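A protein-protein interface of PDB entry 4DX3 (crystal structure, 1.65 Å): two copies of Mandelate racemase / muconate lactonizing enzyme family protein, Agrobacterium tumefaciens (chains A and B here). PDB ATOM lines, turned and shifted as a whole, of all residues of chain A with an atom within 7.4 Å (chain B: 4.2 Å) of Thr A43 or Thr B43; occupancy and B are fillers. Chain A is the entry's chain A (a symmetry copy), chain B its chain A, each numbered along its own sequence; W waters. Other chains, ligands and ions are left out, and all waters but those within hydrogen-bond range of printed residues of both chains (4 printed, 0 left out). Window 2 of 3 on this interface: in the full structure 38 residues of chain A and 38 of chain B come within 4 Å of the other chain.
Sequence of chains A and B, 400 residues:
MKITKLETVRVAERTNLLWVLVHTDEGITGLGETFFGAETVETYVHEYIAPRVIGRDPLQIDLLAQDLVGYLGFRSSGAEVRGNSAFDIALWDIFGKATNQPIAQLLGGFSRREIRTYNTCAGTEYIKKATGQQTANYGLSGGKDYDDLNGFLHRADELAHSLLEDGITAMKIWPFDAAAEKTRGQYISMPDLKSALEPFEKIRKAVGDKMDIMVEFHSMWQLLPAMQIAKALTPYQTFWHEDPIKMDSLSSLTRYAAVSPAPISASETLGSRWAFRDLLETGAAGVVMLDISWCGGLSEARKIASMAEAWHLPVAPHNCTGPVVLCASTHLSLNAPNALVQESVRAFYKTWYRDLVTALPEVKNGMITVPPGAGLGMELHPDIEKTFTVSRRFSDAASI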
ATOM      1  N   THR A   8      -9.504  31.677 -22.861  1.00  0.00           N
ATOM      2  CA  THR A   8      -8.049  31.751 -22.883  1.00  0.00           C
ATOM      3  C   THR A   8      -7.636  33.190 -23.156  1.00  0.00           C
ATOM      4  O   THR A   8      -8.300  33.901 -23.920  1.00  0.00           O
ATOM      5  CB  THR A   8      -7.419  30.809 -23.928  1.00  0.00           C
ATOM      6  OG1 THR A   8      -8.029  31.024 -25.206  1.00  0.00           O
ATOM      7  CG2 THR A   8      -7.575  29.342 -23.512  1.00  0.00           C
ATOM      8  N   ARG A  10      -4.140  35.743 -23.954  1.00  0.00           N
ATOM      9  CA  ARG A  10      -2.720  35.931 -24.247  1.00  0.00           C
ATOM     10  C   ARG A  10      -2.409  37.422 -24.351  1.00  0.00           C
ATOM     11  O   ARG A  10      -3.302  38.237 -24.609  1.00  0.00           O
ATOM     12  CB  ARG A  10      -2.329  35.232 -25.554  1.00  0.00           C
ATOM     13  CG  ARG A  10      -2.431  33.716 -25.488  1.00  0.00           C
ATOM     14  CD  ARG A  10      -1.912  33.037 -26.757  1.00  0.00           C
ATOM     15  NE  ARG A  10      -2.798  33.242 -27.898  1.00  0.00           N
ATOM     16  CZ  ARG A  10      -2.526  34.044 -28.921  1.00  0.00           C
ATOM     17  NH1 ARG A  10      -1.380  34.709 -28.960  1.00  0.00           N
ATOM     18  NH2 ARG A  10      -3.396  34.174 -29.912  1.00  0.00           N
ATOM     19  N   LEU A  18       0.189  31.944 -21.154  1.00  0.00           N
ATOM     20  CA  LEU A  18      -1.209  31.660 -21.464  1.00  0.00           C
ATOM     21  C   LEU A  18      -2.019  31.578 -20.178  1.00  0.00           C
ATOM     22  O   LEU A  18      -1.615  30.897 -19.234  1.00  0.00           O
ATOM     23  CB  LEU A  18      -1.334  30.350 -22.248  1.00  0.00           C
ATOM     24  CG  LEU A  18      -2.779  29.921 -22.528  1.00  0.00           C
ATOM     25  CD1 LEU A  18      -3.413  30.838 -23.563  1.00  0.00           C
ATOM     26  CD2 LEU A  18      -2.845  28.484 -22.995  1.00  0.00           C
ATOM     27  N   GLY A  37       4.709  27.846 -25.758  1.00  0.00           N
ATOM     28  CA  GLY A  37       3.805  27.371 -26.790  1.00  0.00           C
ATOM     29  C   GLY A  37       2.385  27.826 -26.536  1.00  0.00           C
ATOM     30  O   GLY A  37       1.438  27.039 -26.632  1.00  0.00           O
ATOM     31  N   ALA A  38       2.236  29.105 -26.207  1.00  0.00           N
ATOM     32  CA  ALA A  38       0.939  29.624 -25.789  1.00  0.00           C
ATOM     33  C   ALA A  38      -0.140  29.439 -26.846  1.00  0.00           C
ATOM     34  O   ALA A  38      -1.272  29.090 -26.514  1.00  0.00           O
ATOM     35  CB  ALA A  38       1.048  31.080 -25.403  1.00  0.00           C
ATOM     36  N   GLU A  39       0.185  29.697 -28.111  1.00  0.00           N
ATOM     37  CA  GLU A  39      -0.827  29.540 -29.150  1.00  0.00           C
ATOM     38  C   GLU A  39      -1.241  28.084 -29.304  1.00  0.00           C
ATOM     39  O   GLU A  39      -2.417  27.778 -29.498  1.00  0.00           O
ATOM     40  CB  GLU A  39      -0.335  30.071 -30.493  1.00  0.00           C
ATOM     41  CG  GLU A  39      -0.183  31.575 -30.568  1.00  0.00           C
ATOM     42  CD  GLU A  39       0.210  32.024 -31.962  1.00  0.00           C
ATOM     43  OE1 GLU A  39      -0.362  31.491 -32.938  1.00  0.00           O
ATOM     44  OE2 GLU A  39       1.095  32.892 -32.079  1.00  0.00           O
ATOM     45  N   THR A  40      -0.259  27.193 -29.242  1.00  0.00           N
ATOM     46  CA  THR A  40      -0.524  25.763 -29.371  1.00  0.00           C
ATOM     47  C   THR A  40      -1.380  25.240 -28.222  1.00  0.00           C
ATOM     48  O   THR A  40      -2.366  24.528 -28.438  1.00  0.00           O
ATOM     49  CB  THR A  40       0.785  24.968 -29.494  1.00  0.00           C
ATOM     50  OG1 THR A  40       1.488  25.415 -30.661  1.00  0.00           O
ATOM     51  CG2 THR A  40       0.498  23.474 -29.601  1.00  0.00           C
ATOM     52  N   VAL A  41      -1.013  25.598 -27.000  1.00  0.00           N
ATOM     53  CA  VAL A  41      -1.783  25.176 -25.842  1.00  0.00           C
ATOM     54  C   VAL A  41      -3.193  25.768 -25.916  1.00  0.00           C
ATOM     55  O   VAL A  41      -4.173  25.095 -25.601  1.00  0.00           O
ATOM     56  CB  VAL A  41      -1.083  25.548 -24.526  1.00  0.00           C
ATOM     57  CG1 VAL A  41      -1.940  25.128 -23.339  1.00  0.00           C
ATOM     58  CG2 VAL A  41       0.288  24.851 -24.438  1.00  0.00           C
ATOM     59  N   GLU A  42      -3.299  27.015 -26.358  1.00  0.00           N
ATOM     60  CA  GLU A  42      -4.615  27.645 -26.493  1.00  0.00           C
ATOM     61  C   GLU A  42      -5.504  26.861 -27.449  1.00  0.00           C
ATOM     62  O   GLU A  42      -6.665  26.592 -27.152  1.00  0.00           O
ATOM     63  CB  GLU A  42      -4.486  29.098 -26.950  1.00  0.00           C
ATOM     64  CG  GLU A  42      -5.829  29.755 -27.255  1.00  0.00           C
ATOM     65  CD  GLU A  42      -5.692  31.229 -27.545  1.00  0.00           C
ATOM     66  OE1 GLU A  42      -4.899  31.584 -28.447  1.00  0.00           O
ATOM     67  OE2 GLU A  42      -6.378  32.034 -26.875  1.00  0.00           O
ATOM     68  N   THR A  43      -4.953  26.472 -28.594  1.00  0.00           N
ATOM     69  CA  THR A  43      -5.714  25.659 -29.535  1.00  0.00           C
ATOM     70  C   THR A  43      -6.220  24.365 -28.886  1.00  0.00           C
ATOM     71  O   THR A  43      -7.380  23.984 -29.070  1.00  0.00           O
ATOM     72  CB  THR A  43      -4.893  25.332 -30.793  1.00  0.00           C
ATOM     73  OG1 THR A  43      -4.527  26.553 -31.450  1.00  0.00           O
ATOM     74  CG2 THR A  43      -5.717  24.483 -31.748  1.00  0.00           C
ATOM     75  N   TYR A  44      -5.351  23.725 -28.108  1.00  0.00           N
ATOM     76  CA  TYR A  44      -5.666  22.480 -27.425  1.00  0.00           C
ATOM     77  C   TYR A  44      -6.787  22.690 -26.416  1.00  0.00           C
ATOM     78  O   TYR A  44      -7.712  21.872 -26.313  1.00  0.00           O
ATOM     79  CB  TYR A  44      -4.414  21.923 -26.732  1.00  0.00           C
ATOM     80  CG  TYR A  44      -4.711  20.815 -25.747  1.00  0.00           C
ATOM     81  CD1 TYR A  44      -4.917  19.515 -26.179  1.00  0.00           C
ATOM     82  CD2 TYR A  44      -4.778  21.071 -24.384  1.00  0.00           C
ATOM     83  CE1 TYR A  44      -5.202  18.490 -25.285  1.00  0.00           C
ATOM     84  CE2 TYR A  44      -5.058  20.056 -23.479  1.00  0.00           C
ATOM     85  CZ  TYR A  44      -5.257  18.760 -23.939  1.00  0.00           C
ATOM     86  OH  TYR A  44      -5.528  17.723 -23.071  1.00  0.00           O
ATOM     87  N   VAL A  45      -6.714  23.790 -25.671  1.00  0.00           N
ATOM     88  CA  VAL A  45      -7.736  24.054 -24.655  1.00  0.00           C
ATOM     89  C   VAL A  45      -9.130  24.071 -25.279  1.00  0.00           C
ATOM     90  O   VAL A  45     -10.072  23.508 -24.729  1.00  0.00           O
ATOM     91  CB  VAL A  45      -7.455  25.373 -23.905  1.00  0.00           C
ATOM     92  CG1 VAL A  45      -8.646  25.773 -23.047  1.00  0.00           C
ATOM     93  CG2 VAL A  45      -6.192  25.237 -23.051  1.00  0.00           C
ATOM     94  N   HIS A  46      -9.256  24.684 -26.452  1.00  0.00           N
ATOM     95  CA  HIS A  46     -10.554  24.779 -27.104  1.00  0.00           C
ATOM     96  C   HIS A  46     -10.927  23.540 -27.922  1.00  0.00           C
ATOM     97  O   HIS A  46     -12.106  23.188 -28.008  1.00  0.00           O
ATOM     98  CB  HIS A  46     -10.620  26.059 -27.943  1.00  0.00           C
ATOM     99  CG  HIS A  46     -10.496  27.300 -27.120  1.00  0.00           C
ATOM    100  ND1 HIS A  46     -11.538  27.792 -26.362  1.00  0.00           N
ATOM    101  CD2 HIS A  46      -9.441  28.117 -26.890  1.00  0.00           C
ATOM    102  CE1 HIS A  46     -11.134  28.872 -25.719  1.00  0.00           C
ATOM    103  NE2 HIS A  46      -9.867  29.091 -26.018  1.00  0.00           N
ATOM    104  N   GLU A  47      -9.925  22.872 -28.492  1.00  0.00           N
ATOM    105  CA  GLU A  47     -10.162  21.702 -29.340  1.00  0.00           C
ATOM    106  C   GLU A  47     -10.463  20.457 -28.509  1.00  0.00           C
ATOM    107  O   GLU A  47     -11.319  19.648 -28.871  1.00  0.00           O
ATOM    108  CB  GLU A  47      -8.953  21.428 -30.259  1.00  0.00           C
ATOM    109  CG  GLU A  47      -9.124  20.203 -31.182  1.00  0.00           C
ATOM    110  CD  GLU A  47      -7.905  19.907 -32.069  1.00  0.00           C
ATOM    111  OE1 GLU A  47      -6.758  20.020 -31.592  1.00  0.00           O
ATOM    112  OE2 GLU A  47      -8.105  19.542 -33.251  1.00  0.00           O
ATOM    113  N   TYR A  48      -9.764  20.321 -27.384  1.00  0.00           N
ATOM    114  CA  TYR A  48      -9.804  19.086 -26.603  1.00  0.00           C
ATOM    115  C   TYR A  48     -10.466  19.233 -25.233  1.00  0.00           C
ATOM    116  O   TYR A  48     -11.344  18.447 -24.887  1.00  0.00           O
ATOM    117  CB  TYR A  48      -8.387  18.528 -26.435  1.00  0.00           C
ATOM    118  CG  TYR A  48      -8.346  17.109 -25.897  1.00  0.00           C
ATOM    119  CD1 TYR A  48      -8.373  16.023 -26.762  1.00  0.00           C
ATOM    120  CD2 TYR A  48      -8.273  16.860 -24.529  1.00  0.00           C
ATOM    121  CE1 TYR A  48      -8.331  14.722 -26.285  1.00  0.00           C
ATOM    122  CE2 TYR A  48      -8.234  15.560 -24.038  1.00  0.00           C
ATOM    123  CZ  TYR A  48      -8.260  14.494 -24.926  1.00  0.00           C
ATOM    124  OH  TYR A  48      -8.221  13.194 -24.461  1.00  0.00           O
ATOM    125  N   ILE A  49     -10.043  20.214 -24.437  1.00  0.00           N
ATOM    126  CA  ILE A  49     -10.585  20.326 -23.081  1.00  0.00           C
ATOM    127  C   ILE A  49     -12.048  20.785 -23.076  1.00  0.00           C
ATOM    128  O   ILE A  49     -12.893  20.164 -22.426  1.00  0.00           O
ATOM    129  CB  ILE A  49      -9.755  21.263 -22.186  1.00  0.00           C
ATOM    130  CG1 ILE A  49      -8.323  20.734 -22.069  1.00  0.00           C
ATOM    131  CG2 ILE A  49     -10.383  21.364 -20.789  1.00  0.00           C
ATOM    132  CD1 ILE A  49      -7.428  21.560 -21.128  1.00  0.00           C
ATOM    133  N   ARG A 393     -10.024  34.129 -26.370  1.00  0.00           N
ATOM    134  CA  ARG A 393     -10.844  33.195 -27.122  1.00  0.00           C
ATOM    135  C   ARG A 393     -11.767  32.438 -26.173  1.00  0.00           C
ATOM    136  O   ARG A 393     -11.371  32.100 -25.059  1.00  0.00           O
ATOM    137  CB  ARG A 393      -9.971  32.234 -27.919  1.00  0.00           C
ATOM    138  CG  ARG A 393     -10.780  31.227 -28.697  1.00  0.00           C
ATOM    139  CD  ARG A 393      -9.925  30.328 -29.564  1.00  0.00           C
ATOM    140  NE  ARG A 393     -10.759  29.295 -30.167  1.00  0.00           N
ATOM    141  CZ  ARG A 393     -10.295  28.222 -30.794  1.00  0.00           C
ATOM    142  NH1 ARG A 393      -8.986  28.030 -30.906  1.00  0.00           N
ATOM    143  NH2 ARG A 393     -11.142  27.338 -31.301  1.00  0.00           N
ATOM    144  N   GLU B  39      -5.851  20.381 -35.235  1.00  0.00           N
ATOM    145  CA  GLU B  39      -5.761  21.832 -35.107  1.00  0.00           C
ATOM    146  C   GLU B  39      -4.598  22.236 -34.213  1.00  0.00           C
ATOM    147  O   GLU B  39      -3.898  23.210 -34.489  1.00  0.00           O
ATOM    148  CB  GLU B  39      -7.054  22.425 -34.555  1.00  0.00           C
ATOM    149  CG  GLU B  39      -8.237  22.367 -35.498  1.00  0.00           C
ATOM    150  CD  GLU B  39      -9.447  23.065 -34.913  1.00  0.00           C
ATOM    151  OE1 GLU B  39      -9.275  24.159 -34.331  1.00  0.00           O
ATOM    152  OE2 GLU B  39     -10.560  22.517 -35.020  1.00  0.00           O
ATOM    153  N   THR B  40      -4.418  21.495 -33.126  1.00  0.00           N
ATOM    154  CA  THR B  40      -3.334  21.777 -32.189  1.00  0.00           C
ATOM    155  C   THR B  40      -1.965  21.579 -32.830  1.00  0.00           C
ATOM    156  O   THR B  40      -1.080  22.434 -32.715  1.00  0.00           O
ATOM    157  CB  THR B  40      -3.476  20.934 -30.913  1.00  0.00           C
ATOM    158  OG1 THR B  40      -4.725  21.253 -30.285  1.00  0.00           O
ATOM    159  CG2 THR B  40      -2.326  21.215 -29.952  1.00  0.00           C
ATOM    160  N   VAL B  41      -1.789  20.458 -33.516  1.00  0.00           N
ATOM    161  CA  VAL B  41      -0.528  20.193 -34.189  1.00  0.00           C
ATOM    162  C   VAL B  41      -0.291  21.247 -35.274  1.00  0.00           C
ATOM    163  O   VAL B  41       0.828  21.724 -35.451  1.00  0.00           O
ATOM    164  CB  VAL B  41      -0.480  18.770 -34.765  1.00  0.00           C
ATOM    165  CG1 VAL B  41       0.837  18.546 -35.499  1.00  0.00           C
ATOM    166  CG2 VAL B  41      -0.616  17.734 -33.633  1.00  0.00           C
ATOM    167  N   GLU B  42      -1.348  21.631 -35.981  1.00  0.00           N
ATOM    168  CA  GLU B  42      -1.214  22.661 -37.015  1.00  0.00           C
ATOM    169  C   GLU B  42      -0.697  23.966 -36.426  1.00  0.00           C
ATOM    170  O   GLU B  42       0.216  24.584 -36.968  1.00  0.00           O
ATOM    171  CB  GLU B  42      -2.540  22.888 -37.740  1.00  0.00           C
ATOM    172  CG  GLU B  42      -2.498  24.057 -38.720  1.00  0.00           C
ATOM    173  CD  GLU B  42      -3.759  24.161 -39.541  1.00  0.00           C
ATOM    174  OE1 GLU B  42      -4.855  24.230 -38.938  1.00  0.00           O
ATOM    175  OE2 GLU B  42      -3.658  24.177 -40.788  1.00  0.00           O
ATOM    176  N   THR B  43      -1.266  24.380 -35.298  1.00  0.00           N
ATOM    177  CA  THR B  43      -0.783  25.585 -34.631  1.00  0.00           C
ATOM    178  C   THR B  43       0.712  25.490 -34.304  1.00  0.00           C
ATOM    179  O   THR B  43       1.463  26.446 -34.523  1.00  0.00           O
ATOM    180  CB  THR B  43      -1.585  25.885 -33.356  1.00  0.00           C
ATOM    181  OG1 THR B  43      -2.963  26.084 -33.699  1.00  0.00           O
ATOM    182  CG2 THR B  43      -1.054  27.144 -32.689  1.00  0.00           C
ATOM    183  N   TYR B  44       1.128  24.326 -33.811  1.00  0.00           N
ATOM    184  CA  TYR B  44       2.511  24.073 -33.440  1.00  0.00           C
ATOM    185  C   TYR B  44       3.420  24.161 -34.659  1.00  0.00           C
ATOM    186  O   TYR B  44       4.509  24.747 -34.598  1.00  0.00           O
ATOM    187  CB  TYR B  44       2.637  22.696 -32.771  1.00  0.00           C
ATOM    188  CG  TYR B  44       4.065  22.216 -32.639  1.00  0.00           C
ATOM    189  CD1 TYR B  44       4.875  22.669 -31.610  1.00  0.00           C
ATOM    190  CD2 TYR B  44       4.599  21.306 -33.540  1.00  0.00           C
ATOM    191  CE1 TYR B  44       6.192  22.244 -31.484  1.00  0.00           C
ATOM    192  CE2 TYR B  44       5.912  20.870 -33.425  1.00  0.00           C
ATOM    193  CZ  TYR B  44       6.701  21.337 -32.381  1.00  0.00           C
ATOM    194  OH  TYR B  44       8.007  20.922 -32.227  1.00  0.00           O
ATOM    195  N   VAL B  45       2.975  23.583 -35.772  1.00  0.00           N
ATOM    196  CA  VAL B  45       3.800  23.596 -36.981  1.00  0.00           C
ATOM    197  C   VAL B  45       4.162  25.026 -37.377  1.00  0.00           C
ATOM    198  O   VAL B  45       5.303  25.310 -37.730  1.00  0.00           O
ATOM    199  CB  VAL B  45       3.099  22.866 -38.146  1.00  0.00           C
ATOM    200  CG1 VAL B  45       3.831  23.109 -39.458  1.00  0.00           C
ATOM    201  CG2 VAL B  45       2.999  21.368 -37.850  1.00  0.00           C
ATOM    202  N   HIS B  46       3.201  25.939 -37.278  1.00  0.00           N
ATOM    203  CA  HIS B  46       3.448  27.320 -37.665  1.00  0.00           C
ATOM    204  C   HIS B  46       4.103  28.162 -36.568  1.00  0.00           C
ATOM    205  O   HIS B  46       4.892  29.062 -36.867  1.00  0.00           O
ATOM    206  CB  HIS B  46       2.149  27.955 -38.174  1.00  0.00           C
ATOM    207  CG  HIS B  46       1.618  27.286 -39.400  1.00  0.00           C
ATOM    208  ND1 HIS B  46       2.161  27.493 -40.650  1.00  0.00           N
ATOM    209  CD2 HIS B  46       0.631  26.373 -39.562  1.00  0.00           C
ATOM    210  CE1 HIS B  46       1.515  26.752 -41.532  1.00  0.00           C
ATOM    211  NE2 HIS B  46       0.585  26.061 -40.900  1.00  0.00           N
ATOM    212  N   GLU B  47       3.798  27.852 -35.309  1.00  0.00           N
ATOM    213  CA  GLU B  47       4.323  28.618 -34.176  1.00  0.00           C
ATOM    214  C   GLU B  47       5.773  28.249 -33.872  1.00  0.00           C
ATOM    215  O   GLU B  47       6.590  29.115 -33.549  1.00  0.00           O
ATOM    216  CB  GLU B  47       3.461  28.404 -32.914  1.00  0.00           C
ATOM    217  CG  GLU B  47       3.955  29.176 -31.672  1.00  0.00           C
ATOM    218  CD  GLU B  47       3.120  28.933 -30.406  1.00  0.00           C
ATOM    219  OE1 GLU B  47       2.712  27.782 -30.152  1.00  0.00           O
ATOM    220  OE2 GLU B  47       2.887  29.907 -29.652  1.00  0.00           O
HETATM  221  O   HOH W   1       4.486  30.916 -26.947  1.00  0.00           O
HETATM  222  O   HOH W   2     -11.498  24.120 -31.918  1.00  0.00           O
HETATM  223  O   HOH W   3      -6.143  18.323 -29.449  1.00  0.00           O
HETATM  224  O   HOH W   4       4.690  25.840 -29.734  1.00  0.00           O
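The side-chain carboxylate (OE2) of Glu A47 lies within hydrogen-bond range of the backbone NH (N) of Glu B39, 3.1 Å away. The side-chain hydroxyl of Thr B40 sits close to the backbone NH of Tyr A44 (3.4 Å). OG1 of Thr B40 lies within hydrogen-bond range of OE1 of Glu A47. OG1 of Thr B43 lies within hydrogen-bond range of OG1 of Thr A43. OG1 of Thr A40 sits close to N of Tyr B44, at 3.4 Å. OE2 of Glu B47 lies within hydrogen-bond range of N of Glu A39 (3.1 Å). OE1 of Glu B47 sits at hydrogen-bond distance from OG1 of Thr A40.
The backbone carbonyl oxygen (O) of Glu B39 is in hydrogen-bond range of the side-chain hydroxyl (OG1) of Thr B43 (3.1 Å). The backbone carbonyl oxygen (O) of Glu A39 lies within hydrogen-bond range of the side-chain hydroxyl (OG1) of Thr A43, at 3.1 Å. O of Tyr A44 is in hydrogen-bond range of N of Ile A49, 3.4 Å away.
OE1 of Glu B47 touches CA of Gly A37 (3.6 Å). N of Ala A38 touches OE2 of Glu B47, at 3.6 Å. Thr B43 touches Glu A39 (CG2 to C, 3.5 Å). Thr A40 touches Thr B40 (CG2 to CG2, 3.6 Å). N of Thr A40 touches CG2 of Thr B43 (3.5 Å). CG2 of Thr A43 touches C of Glu B39, at 3.5 Å. CG2 of Thr A43 touches N of Thr B40 (3.5 Å).
Thr A43 touches just these residues of chain B: Glu B39, Thr B40 and Thr B43. Thr B43 touches just these residues of chain A: Glu A39 (3.5 Å), Thr A40 (3.5 Å) and Thr A43 (2.8 Å). Printed residues of chain B within 4 Å of Ala A38: Glu B47 (3.6 Å). Of the printed residues of chain B, Gly A37 touches Glu B47 (3.6 Å). The nearest printed residue of chain B that does not touch Thr A43 is Val B41 (5.9 Å).
Hydrophobic or aromatic side chains of chain B within 4 Å of the printed part of chain A: Tyr B44. Of the 17 printed residues of chain A, 7 touch a printed residue of chain B. Printed residues of chain A that touch a printed residue of chain B: Gly A37, Ala A38, Glu A39, Thr A40, Thr A43, Tyr A44 and Glu A47. Among the printed residues, 14 pairs touch across the chains. Among the printed residues, no Asp or Glu carboxylate lies within 4 Å of a Lys or Arg side-chain nitrogen of the other chain.
Glu A39 touches Thr B43, and with the chains exchanged Thr A43 touches Glu B39. Thr A40 touches its own counterpart, Thr B40. Thr A40 touches Thr B43, and with the chains exchanged Thr A43 touches Thr B40. Thr A40 touches Glu B47, and with the chains exchanged Glu A47 touches Thr B40. Positions printed for both chains: 39, 40, 41, 42, 43, 44, 45, 46 and 47. Of the 14 pairs that touch across the chains among the printed residues, 12 have their exchanged pair printed and touching as well.
Water W4 bridges OE1 of Glu B47 (2.8 Å) and OG1 of Thr A40 (3.4 Å). Water W3 lies within hydrogen-bond range of the side-chain carboxylate (OE1) of Glu A47 (2.8 Å) and the side-chain hydroxyl (OG1) of Thr B40 (3.4 Å). Water W1 lies within hydrogen-bond range of the backbone NH (N) of Ala A38, the backbone NH (N) of Gly A37 and the side-chain carboxylate (OE2) of Glu B47. Water W2 lies within hydrogen-bond range of OE1 of Glu B39 and NH2 of Arg A393.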
